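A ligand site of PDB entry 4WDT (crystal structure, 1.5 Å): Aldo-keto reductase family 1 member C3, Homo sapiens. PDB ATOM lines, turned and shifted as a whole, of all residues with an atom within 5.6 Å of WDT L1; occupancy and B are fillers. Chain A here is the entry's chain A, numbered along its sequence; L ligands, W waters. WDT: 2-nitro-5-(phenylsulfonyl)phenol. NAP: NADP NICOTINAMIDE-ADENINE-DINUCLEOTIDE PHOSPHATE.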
ATOM      1  N   TYR A  24     -26.797 -11.368 -19.835  1.00  0.00           N
ATOM      2  CA  TYR A  24     -26.737 -12.775 -19.538  1.00  0.00           C
ATOM      3  C   TYR A  24     -27.495 -13.118 -18.272  1.00  0.00           C
ATOM      4  O   TYR A  24     -27.351 -12.431 -17.245  1.00  0.00           O
ATOM      5  CB  TYR A  24     -25.285 -13.242 -19.348  1.00  0.00           C
ATOM      6  CG  TYR A  24     -25.227 -14.704 -19.103  1.00  0.00           C
ATOM      7  CD1 TYR A  24     -25.415 -15.620 -20.115  1.00  0.00           C
ATOM      8  CD2 TYR A  24     -25.056 -15.197 -17.824  1.00  0.00           C
ATOM      9  CE1 TYR A  24     -25.416 -16.991 -19.867  1.00  0.00           C
ATOM     10  CE2 TYR A  24     -25.100 -16.595 -17.596  1.00  0.00           C
ATOM     11  CZ  TYR A  24     -25.220 -17.448 -18.650  1.00  0.00           C
ATOM     12  OH  TYR A  24     -25.201 -18.846 -18.429  1.00  0.00           O
ATOM     13  N   LEU A  54     -23.993 -17.120 -27.250  1.00  0.00           N
ATOM     14  CA  LEU A  54     -23.922 -17.947 -26.066  1.00  0.00           C
ATOM     15  C   LEU A  54     -25.108 -17.767 -25.156  1.00  0.00           C
ATOM     16  O   LEU A  54     -25.544 -18.710 -24.464  1.00  0.00           O
ATOM     17  CB  LEU A  54     -22.594 -17.608 -25.296  1.00  0.00           C
ATOM     18  CG  LEU A  54     -22.392 -18.434 -24.030  1.00  0.00           C
ATOM     19  CD1 LEU A  54     -22.205 -19.944 -24.410  1.00  0.00           C
ATOM     20  CD2 LEU A  54     -21.281 -17.879 -23.181  1.00  0.00           C
ATOM     21  N   TYR A  55     -25.648 -16.532 -25.088  1.00  0.00           N
ATOM     22  CA  TYR A  55     -26.620 -16.174 -24.047  1.00  0.00           C
ATOM     23  C   TYR A  55     -27.983 -16.763 -24.255  1.00  0.00           C
ATOM     24  O   TYR A  55     -28.772 -16.727 -23.347  1.00  0.00           O
ATOM     25  CB  TYR A  55     -26.692 -14.673 -23.797  1.00  0.00           C
ATOM     26  CG  TYR A  55     -25.382 -14.036 -23.441  1.00  0.00           C
ATOM     27  CD1 TYR A  55     -25.290 -12.622 -23.476  1.00  0.00           C
ATOM     28  CD2 TYR A  55     -24.260 -14.783 -23.127  1.00  0.00           C
ATOM     29  CE1 TYR A  55     -24.072 -12.009 -23.225  1.00  0.00           C
ATOM     30  CE2 TYR A  55     -23.017 -14.155 -22.855  1.00  0.00           C
ATOM     31  CZ  TYR A  55     -22.947 -12.770 -22.915  1.00  0.00           C
ATOM     32  OH  TYR A  55     -21.788 -12.078 -22.701  1.00  0.00           O
ATOM     33  N   LYS A  84     -21.846 -11.424 -30.134  1.00  0.00           N
ATOM     34  CA  LYS A  84     -20.459 -12.016 -30.102  1.00  0.00           C
ATOM     35  C   LYS A  84     -20.466 -13.404 -30.758  1.00  0.00           C
ATOM     36  O   LYS A  84     -21.485 -14.149 -30.690  1.00  0.00           O
ATOM     37  CB  LYS A  84     -20.007 -12.220 -28.655  1.00  0.00           C
ATOM     38  CG  LYS A  84     -20.234 -11.010 -27.757  1.00  0.00           C
ATOM     39  CD  LYS A  84     -19.596 -11.220 -26.365  1.00  0.00           C
ATOM     40  CE  LYS A  84     -19.948 -10.090 -25.369  1.00  0.00           C
ATOM     41  NZ  LYS A  84     -21.310 -10.270 -24.819  1.00  0.00           N
ATOM     42  N   TRP A  86     -19.451 -16.969 -31.188  1.00  0.00           N
ATOM     43  CA  TRP A  86     -19.105 -17.999 -30.205  1.00  0.00           C
ATOM     44  C   TRP A  86     -17.898 -18.832 -30.649  1.00  0.00           C
ATOM     45  O   TRP A  86     -17.548 -18.847 -31.851  1.00  0.00           O
ATOM     46  CB  TRP A  86     -20.382 -18.797 -29.878  1.00  0.00           C
ATOM     47  CG  TRP A  86     -20.075 -19.875 -28.794  1.00  0.00           C
ATOM     48  CD1 TRP A  86     -20.161 -21.289 -28.995  1.00  0.00           C
ATOM     49  CD2 TRP A  86     -19.493 -19.685 -27.507  1.00  0.00           C
ATOM     50  NE1 TRP A  86     -19.711 -21.897 -27.849  1.00  0.00           N
ATOM     51  CE2 TRP A  86     -19.270 -20.992 -26.929  1.00  0.00           C
ATOM     52  CE3 TRP A  86     -19.064 -18.535 -26.779  1.00  0.00           C
ATOM     53  CZ2 TRP A  86     -18.674 -21.163 -25.641  1.00  0.00           C
ATOM     54  CZ3 TRP A  86     -18.564 -18.699 -25.545  1.00  0.00           C
ATOM     55  CH2 TRP A  86     -18.316 -20.029 -24.970  1.00  0.00           C
ATOM     56  N   HIS A 117     -15.887 -13.639 -29.035  1.00  0.00           N
ATOM     57  CA  HIS A 117     -16.298 -13.745 -27.636  1.00  0.00           C
ATOM     58  C   HIS A 117     -15.132 -14.156 -26.747  1.00  0.00           C
ATOM     59  O   HIS A 117     -14.982 -13.688 -25.580  1.00  0.00           O
ATOM     60  CB  HIS A 117     -17.408 -14.787 -27.504  1.00  0.00           C
ATOM     61  CG  HIS A 117     -18.271 -14.691 -26.270  1.00  0.00           C
ATOM     62  ND1 HIS A 117     -19.601 -15.008 -26.343  1.00  0.00           N
ATOM     63  CD2 HIS A 117     -18.033 -14.231 -24.992  1.00  0.00           C
ATOM     64  CE1 HIS A 117     -20.175 -14.805 -25.166  1.00  0.00           C
ATOM     65  NE2 HIS A 117     -19.236 -14.307 -24.330  1.00  0.00           N
ATOM     66  N   SER A 118     -14.255 -15.036 -27.263  1.00  0.00           N
ATOM     67  CA  SER A 118     -13.105 -15.499 -26.478  1.00  0.00           C
ATOM     68  C   SER A 118     -12.042 -15.985 -27.434  1.00  0.00           C
ATOM     69  O   SER A 118     -12.354 -16.466 -28.542  1.00  0.00           O
ATOM     70  CB  SER A 118     -13.651 -16.584 -25.580  1.00  0.00           C
ATOM     71  OG  SER A 118     -12.732 -17.578 -25.201  1.00  0.00           O
ATOM     72  N   MET A 120     -10.491 -18.686 -26.907  1.00  0.00           N
ATOM     73  CA  MET A 120     -10.356 -20.134 -26.650  1.00  0.00           C
ATOM     74  C   MET A 120     -11.244 -20.917 -27.616  1.00  0.00           C
ATOM     75  O   MET A 120     -12.331 -21.380 -27.244  1.00  0.00           O
ATOM     76  CB  MET A 120     -10.736 -20.383 -25.220  1.00  0.00           C
ATOM     77  CG  MET A 120      -9.676 -19.817 -24.249  1.00  0.00           C
ATOM     78  SD  MET A 120     -10.129 -20.145 -22.531  1.00  0.00           S
ATOM     79  CE  MET A 120     -11.088 -18.616 -22.365  1.00  0.00           C
ATOM     80  N   ASN A 167     -12.055 -11.078 -23.972  1.00  0.00           N
ATOM     81  CA  ASN A 167     -11.221 -12.088 -23.238  1.00  0.00           C
ATOM     82  C   ASN A 167      -9.820 -12.244 -23.846  1.00  0.00           C
ATOM     83  O   ASN A 167      -9.187 -13.267 -23.573  1.00  0.00           O
ATOM     84  CB  ASN A 167     -11.952 -13.455 -23.115  1.00  0.00           C
ATOM     85  CG  ASN A 167     -13.159 -13.329 -22.273  1.00  0.00           C
ATOM     86  OD1 ASN A 167     -13.008 -12.974 -21.040  1.00  0.00           O
ATOM     87  ND2 ASN A 167     -14.335 -13.553 -22.833  1.00  0.00           N
ATOM     88  N   TYR A 216     -16.538  -6.352 -17.958  1.00  0.00           N
ATOM     89  CA  TYR A 216     -17.630  -7.227 -17.550  1.00  0.00           C
ATOM     90  C   TYR A 216     -17.376  -7.769 -16.151  1.00  0.00           C
ATOM     91  O   TYR A 216     -16.249  -7.795 -15.649  1.00  0.00           O
ATOM     92  CB  TYR A 216     -17.879  -8.371 -18.566  1.00  0.00           C
ATOM     93  CG  TYR A 216     -16.891  -9.523 -18.634  1.00  0.00           C
ATOM     94  CD1 TYR A 216     -16.121  -9.759 -19.775  1.00  0.00           C
ATOM     95  CD2 TYR A 216     -16.796 -10.475 -17.584  1.00  0.00           C
ATOM     96  CE1 TYR A 216     -15.272 -10.914 -19.867  1.00  0.00           C
ATOM     97  CE2 TYR A 216     -16.016 -11.591 -17.680  1.00  0.00           C
ATOM     98  CZ  TYR A 216     -15.234 -11.771 -18.828  1.00  0.00           C
ATOM     99  OH  TYR A 216     -14.418 -12.900 -18.872  1.00  0.00           O
ATOM    100  N   GLN A 222     -21.986 -13.096 -11.535  1.00  0.00           N
ATOM    101  CA  GLN A 222     -23.138 -13.734 -11.018  1.00  0.00           C
ATOM    102  C   GLN A 222     -22.766 -15.004 -10.186  1.00  0.00           C
ATOM    103  O   GLN A 222     -23.663 -15.645  -9.649  1.00  0.00           O
ATOM    104  CB  GLN A 222     -24.108 -14.076 -12.155  1.00  0.00           C
ATOM    105  CG  GLN A 222     -24.507 -12.840 -12.904  1.00  0.00           C
ATOM    106  CD  GLN A 222     -25.572 -13.115 -13.974  1.00  0.00           C
ATOM    107  OE1 GLN A 222     -26.640 -13.744 -13.667  1.00  0.00           O
ATOM    108  NE2 GLN A 222     -25.377 -12.623 -15.227  1.00  0.00           N
ATOM    109  N   TRP A 227     -18.485 -22.004 -12.851  1.00  0.00           N
ATOM    110  CA  TRP A 227     -17.234 -21.325 -13.139  1.00  0.00           C
ATOM    111  C   TRP A 227     -16.577 -20.654 -11.956  1.00  0.00           C
ATOM    112  O   TRP A 227     -15.391 -20.327 -12.081  1.00  0.00           O
ATOM    113  CB  TRP A 227     -17.455 -20.236 -14.255  1.00  0.00           C
ATOM    114  CG  TRP A 227     -18.086 -20.847 -15.478  1.00  0.00           C
ATOM    115  CD1 TRP A 227     -17.638 -21.957 -16.199  1.00  0.00           C
ATOM    116  CD2 TRP A 227     -19.296 -20.463 -16.054  1.00  0.00           C
ATOM    117  NE1 TRP A 227     -18.527 -22.217 -17.231  1.00  0.00           N
ATOM    118  CE2 TRP A 227     -19.522 -21.291 -17.187  1.00  0.00           C
ATOM    119  CE3 TRP A 227     -20.171 -19.410 -15.816  1.00  0.00           C
ATOM    120  CZ2 TRP A 227     -20.656 -21.111 -18.017  1.00  0.00           C
ATOM    121  CZ3 TRP A 227     -21.329 -19.257 -16.589  1.00  0.00           C
ATOM    122  CH2 TRP A 227     -21.533 -20.086 -17.728  1.00  0.00           C
ATOM    123  N   PHE A 306     -14.182 -16.024 -13.008  1.00  0.00           N
ATOM    124  CA  PHE A 306     -14.243 -17.208 -13.939  1.00  0.00           C
ATOM    125  C   PHE A 306     -12.952 -17.925 -13.811  1.00  0.00           C
ATOM    126  O   PHE A 306     -11.920 -17.436 -14.249  1.00  0.00           O
ATOM    127  CB  PHE A 306     -14.434 -16.678 -15.386  1.00  0.00           C
ATOM    128  CG  PHE A 306     -15.893 -16.185 -15.630  1.00  0.00           C
ATOM    129  CD1 PHE A 306     -16.228 -14.805 -15.272  1.00  0.00           C
ATOM    130  CD2 PHE A 306     -16.886 -17.011 -16.148  1.00  0.00           C
ATOM    131  CE1 PHE A 306     -17.536 -14.319 -15.412  1.00  0.00           C
ATOM    132  CE2 PHE A 306     -18.211 -16.471 -16.372  1.00  0.00           C
ATOM    133  CZ  PHE A 306     -18.538 -15.165 -15.981  1.00  0.00           C
ATOM    134  N   PHE A 311     -11.727 -24.613 -18.672  1.00  0.00           N
ATOM    135  CA  PHE A 311     -10.960 -23.873 -19.668  1.00  0.00           C
ATOM    136  C   PHE A 311      -9.493 -23.457 -19.274  1.00  0.00           C
ATOM    137  O   PHE A 311      -8.756 -22.918 -20.114  1.00  0.00           O
ATOM    138  CB  PHE A 311     -11.757 -22.594 -20.038  1.00  0.00           C
ATOM    139  CG  PHE A 311     -12.355 -21.892 -18.884  1.00  0.00           C
ATOM    140  CD1 PHE A 311     -11.577 -21.012 -18.109  1.00  0.00           C
ATOM    141  CD2 PHE A 311     -13.708 -22.077 -18.577  1.00  0.00           C
ATOM    142  CE1 PHE A 311     -12.151 -20.355 -16.994  1.00  0.00           C
ATOM    143  CE2 PHE A 311     -14.272 -21.406 -17.478  1.00  0.00           C
ATOM    144  CZ  PHE A 311     -13.481 -20.537 -16.706  1.00  0.00           C
ATOM    145  N   TYR A 319      -5.316 -16.106 -19.214  1.00  0.00           N
ATOM    146  CA  TYR A 319      -4.768 -15.743 -17.905  1.00  0.00           C
ATOM    147  C   TYR A 319      -3.460 -16.585 -17.618  1.00  0.00           C
ATOM    148  O   TYR A 319      -3.374 -17.762 -17.993  1.00  0.00           O
ATOM    149  CB  TYR A 319      -5.819 -15.957 -16.754  1.00  0.00           C
ATOM    150  CG  TYR A 319      -7.109 -15.139 -16.928  1.00  0.00           C
ATOM    151  CD1 TYR A 319      -7.060 -13.834 -17.410  1.00  0.00           C
ATOM    152  CD2 TYR A 319      -8.360 -15.726 -16.622  1.00  0.00           C
ATOM    153  CE1 TYR A 319      -8.211 -13.103 -17.591  1.00  0.00           C
ATOM    154  CE2 TYR A 319      -9.567 -15.001 -16.827  1.00  0.00           C
ATOM    155  CZ  TYR A 319      -9.435 -13.670 -17.278  1.00  0.00           C
ATOM    156  OH  TYR A 319     -10.570 -12.934 -17.434  1.00  0.00           O
HETATM  157  C17 WDT L   1     -13.609 -17.164 -19.035  1.00  0.00           C
HETATM  158  C14 WDT L   1     -14.139 -18.445 -19.109  1.00  0.00           C
HETATM  159  C15 WDT L   1     -14.336 -16.205 -19.675  1.00  0.00           C
HETATM  160  C9  WDT L   1     -20.395 -16.469 -19.047  1.00  0.00           C
HETATM  161  C10 WDT L   1     -15.310 -18.734 -19.760  1.00  0.00           C
HETATM  162  C11 WDT L   1     -15.518 -16.458 -20.362  1.00  0.00           C
HETATM  163  C4  WDT L   1     -19.468 -17.441 -19.449  1.00  0.00           C
HETATM  164  C3  WDT L   1     -18.920 -16.121 -21.454  1.00  0.00           C
HETATM  165  C12 WDT L   1     -20.608 -15.366 -19.848  1.00  0.00           C
HETATM  166  C8  WDT L   1     -19.860 -15.209 -21.033  1.00  0.00           C
HETATM  167  C5  WDT L   1     -16.016 -17.738 -20.381  1.00  0.00           C
HETATM  168  C1  WDT L   1     -18.758 -17.198 -20.622  1.00  0.00           C
HETATM  169  N16 WDT L   1     -21.504 -14.397 -19.318  1.00  0.00           N
HETATM  170  O19 WDT L   1     -21.839 -14.318 -18.089  1.00  0.00           O
HETATM  171  O18 WDT L   1     -21.822 -13.370 -19.960  1.00  0.00           O
HETATM  172  O6  WDT L   1     -17.157 -18.082 -22.568  1.00  0.00           O
HETATM  173  O7  WDT L   1     -17.919 -19.503 -20.525  1.00  0.00           O
HETATM  174  O13 WDT L   1     -20.040 -14.113 -21.774  1.00  0.00           O
HETATM  175  S2  WDT L   1     -17.516 -18.273 -21.201  1.00  0.00           S
HETATM  176  PA  NAP L   2     -22.338  -8.130 -13.090  1.00  0.00           P
HETATM  177  O1A NAP L   2     -20.956  -8.259 -12.521  1.00  0.00           O
HETATM  178  O2A NAP L   2     -22.644  -6.936 -13.922  1.00  0.00           O
HETATM  179  O5B NAP L   2     -23.435  -8.127 -11.960  1.00  0.00           O
HETATM  180  C5B NAP L   2     -23.372  -9.189 -10.973  1.00  0.00           C
HETATM  181  C4B NAP L   2     -24.632  -9.215 -10.141  1.00  0.00           C
HETATM  182  O4B NAP L   2     -24.771  -7.921  -9.563  1.00  0.00           O
HETATM  183  C3B NAP L   2     -25.913  -9.389 -10.935  1.00  0.00           C
HETATM  184  O3B NAP L   2     -26.254 -10.807 -11.010  1.00  0.00           O
HETATM  185  C2B NAP L   2     -26.965  -8.530 -10.275  1.00  0.00           C
HETATM  186  O2B NAP L   2     -27.979  -9.257  -9.613  1.00  0.00           O
HETATM  187  C1B NAP L   2     -26.129  -7.808  -9.169  1.00  0.00           C
HETATM  188  N9A NAP L   2     -26.443  -6.354  -9.157  1.00  0.00           N
HETATM  189  C8A NAP L   2     -26.634  -5.496 -10.273  1.00  0.00           C
HETATM  190  N7A NAP L   2     -26.805  -4.242  -9.894  1.00  0.00           N
HETATM  191  C5A NAP L   2     -26.715  -4.266  -8.506  1.00  0.00           C
HETATM  192  C6A NAP L   2     -26.837  -3.250  -7.596  1.00  0.00           C
HETATM  193  N6A NAP L   2     -27.127  -1.978  -7.911  1.00  0.00           N
HETATM  194  N1A NAP L   2     -26.706  -3.623  -6.327  1.00  0.00           N
HETATM  195  C2A NAP L   2     -26.446  -4.883  -5.968  1.00  0.00           C
HETATM  196  N3A NAP L   2     -26.312  -5.963  -6.753  1.00  0.00           N
HETATM  197  C4A NAP L   2     -26.470  -5.541  -8.035  1.00  0.00           C
HETATM  198  O3  NAP L   2     -22.692  -9.474 -13.935  1.00  0.00           O
HETATM  199  PN  NAP L   2     -22.116 -10.255 -15.180  1.00  0.00           P
HETATM  200  O1N NAP L   2     -20.992 -11.132 -14.731  1.00  0.00           O
HETATM  201  O2N NAP L   2     -23.327 -10.875 -15.851  1.00  0.00           O
HETATM  202  O5D NAP L   2     -21.469  -9.155 -16.084  1.00  0.00           O
HETATM  203  C5D NAP L   2     -22.310  -8.218 -16.824  1.00  0.00           C
HETATM  204  C4D NAP L   2     -22.480  -8.584 -18.305  1.00  0.00           C
HETATM  205  O4D NAP L   2     -21.203  -8.645 -18.952  1.00  0.00           O
HETATM  206  C3D NAP L   2     -23.092  -9.902 -18.664  1.00  0.00           C
HETATM  207  O3D NAP L   2     -24.536  -9.950 -18.389  1.00  0.00           O
HETATM  208  C2D NAP L   2     -22.713 -10.028 -20.114  1.00  0.00           C
HETATM  209  O2D NAP L   2     -23.488  -9.134 -20.836  1.00  0.00           O
HETATM  210  C1D NAP L   2     -21.259  -9.553 -20.029  1.00  0.00           C
HETATM  211  N1N NAP L   2     -20.270 -10.639 -19.792  1.00  0.00           N
HETATM  212  C2N NAP L   2     -19.452 -10.949 -20.831  1.00  0.00           C
HETATM  213  C3N NAP L   2     -18.517 -11.954 -20.666  1.00  0.00           C
HETATM  214  C7N NAP L   2     -17.549 -12.320 -21.740  1.00  0.00           C
HETATM  215  O7N NAP L   2     -16.898 -13.359 -21.690  1.00  0.00           O
HETATM  216  N7N NAP L   2     -17.358 -11.411 -22.725  1.00  0.00           N
HETATM  217  C4N NAP L   2     -18.468 -12.631 -19.444  1.00  0.00           C
HETATM  218  C5N NAP L   2     -19.332 -12.283 -18.415  1.00  0.00           C
HETATM  219  C6N NAP L   2     -20.198 -11.263 -18.582  1.00  0.00           C
HETATM  220  P2B NAP L   2     -29.539  -8.958  -9.972  1.00  0.00           P
HETATM  221  O1X NAP L   2     -29.783  -9.401 -11.416  1.00  0.00           O
HETATM  222  O2X NAP L   2     -30.238  -9.858  -8.901  1.00  0.00           O
HETATM  223  O3X NAP L   2     -29.716  -7.493  -9.728  1.00  0.00           O
HETATM  224  O   HOH W   1     -22.407 -15.738 -15.331  1.00  0.00           O
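The backbone carbonyl oxygen (O) of His 117 lies within hydrogen-bond range of the side-chain amide nitrogen (ND2) of Asn 167 (2.8 Å). NZ of Lys 84 lies within hydrogen-bond range of OH of Tyr 55, 2.8 Å away. The side-chain amide nitrogen of Gln 222 is in hydrogen-bond range of the backbone carbonyl oxygen of Tyr 24 (2.8 Å). OH of Tyr 216 is in hydrogen-bond range of OD1 of Asn 167 (2.6 Å).
Residues that only touch WDT L1: Tyr 24 (3.3 Å), Leu 54 (3.4 Å), Trp 86 (3.3 Å), Asn 167 (3.8 Å), Tyr 216 (3.4 Å), Trp 227 (3.8 Å), Phe 306 (3.5 Å) and Phe 311 (3.3 Å). Hydrophobic or aromatic side chains within 4 Å of WDT L1: Tyr 24, Leu 54, Tyr 55, Trp 86, His 117, Trp 227, Phe 306 and Phe 311. Ten residues have an atom within 4 Å of WDT L1: Tyr 24, Leu 54, Tyr 55, Trp 86, His 117, Asn 167, Tyr 216, Trp 227, Phe 306 and Phe 311. The nearest printed residue that does not touch WDT L1 is Met 120 (4.4 Å).
An oxygen (O7N) of NAP L2 lies close to an oxygen (O13) of WDT L1, at 3.2 Å.
A ring nitrogen (NE2) of His 117 is in hydrogen-bond range of an oxygen (O13) of WDT L1, 2.7 Å away. OH of Tyr 55 is in hydrogen-bond range of O13 of WDT L1 (2.8 Å). O3D of NAP L2 lies within hydrogen-bond range of N of Tyr 24 (3.0 Å). ND2 of Asn 167 sits at hydrogen-bond distance from O7N of NAP L2 (2.8 Å). The side-chain amide nitrogen of Gln 222 lies within hydrogen-bond range of an oxygen (O2N) of NAP L2.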
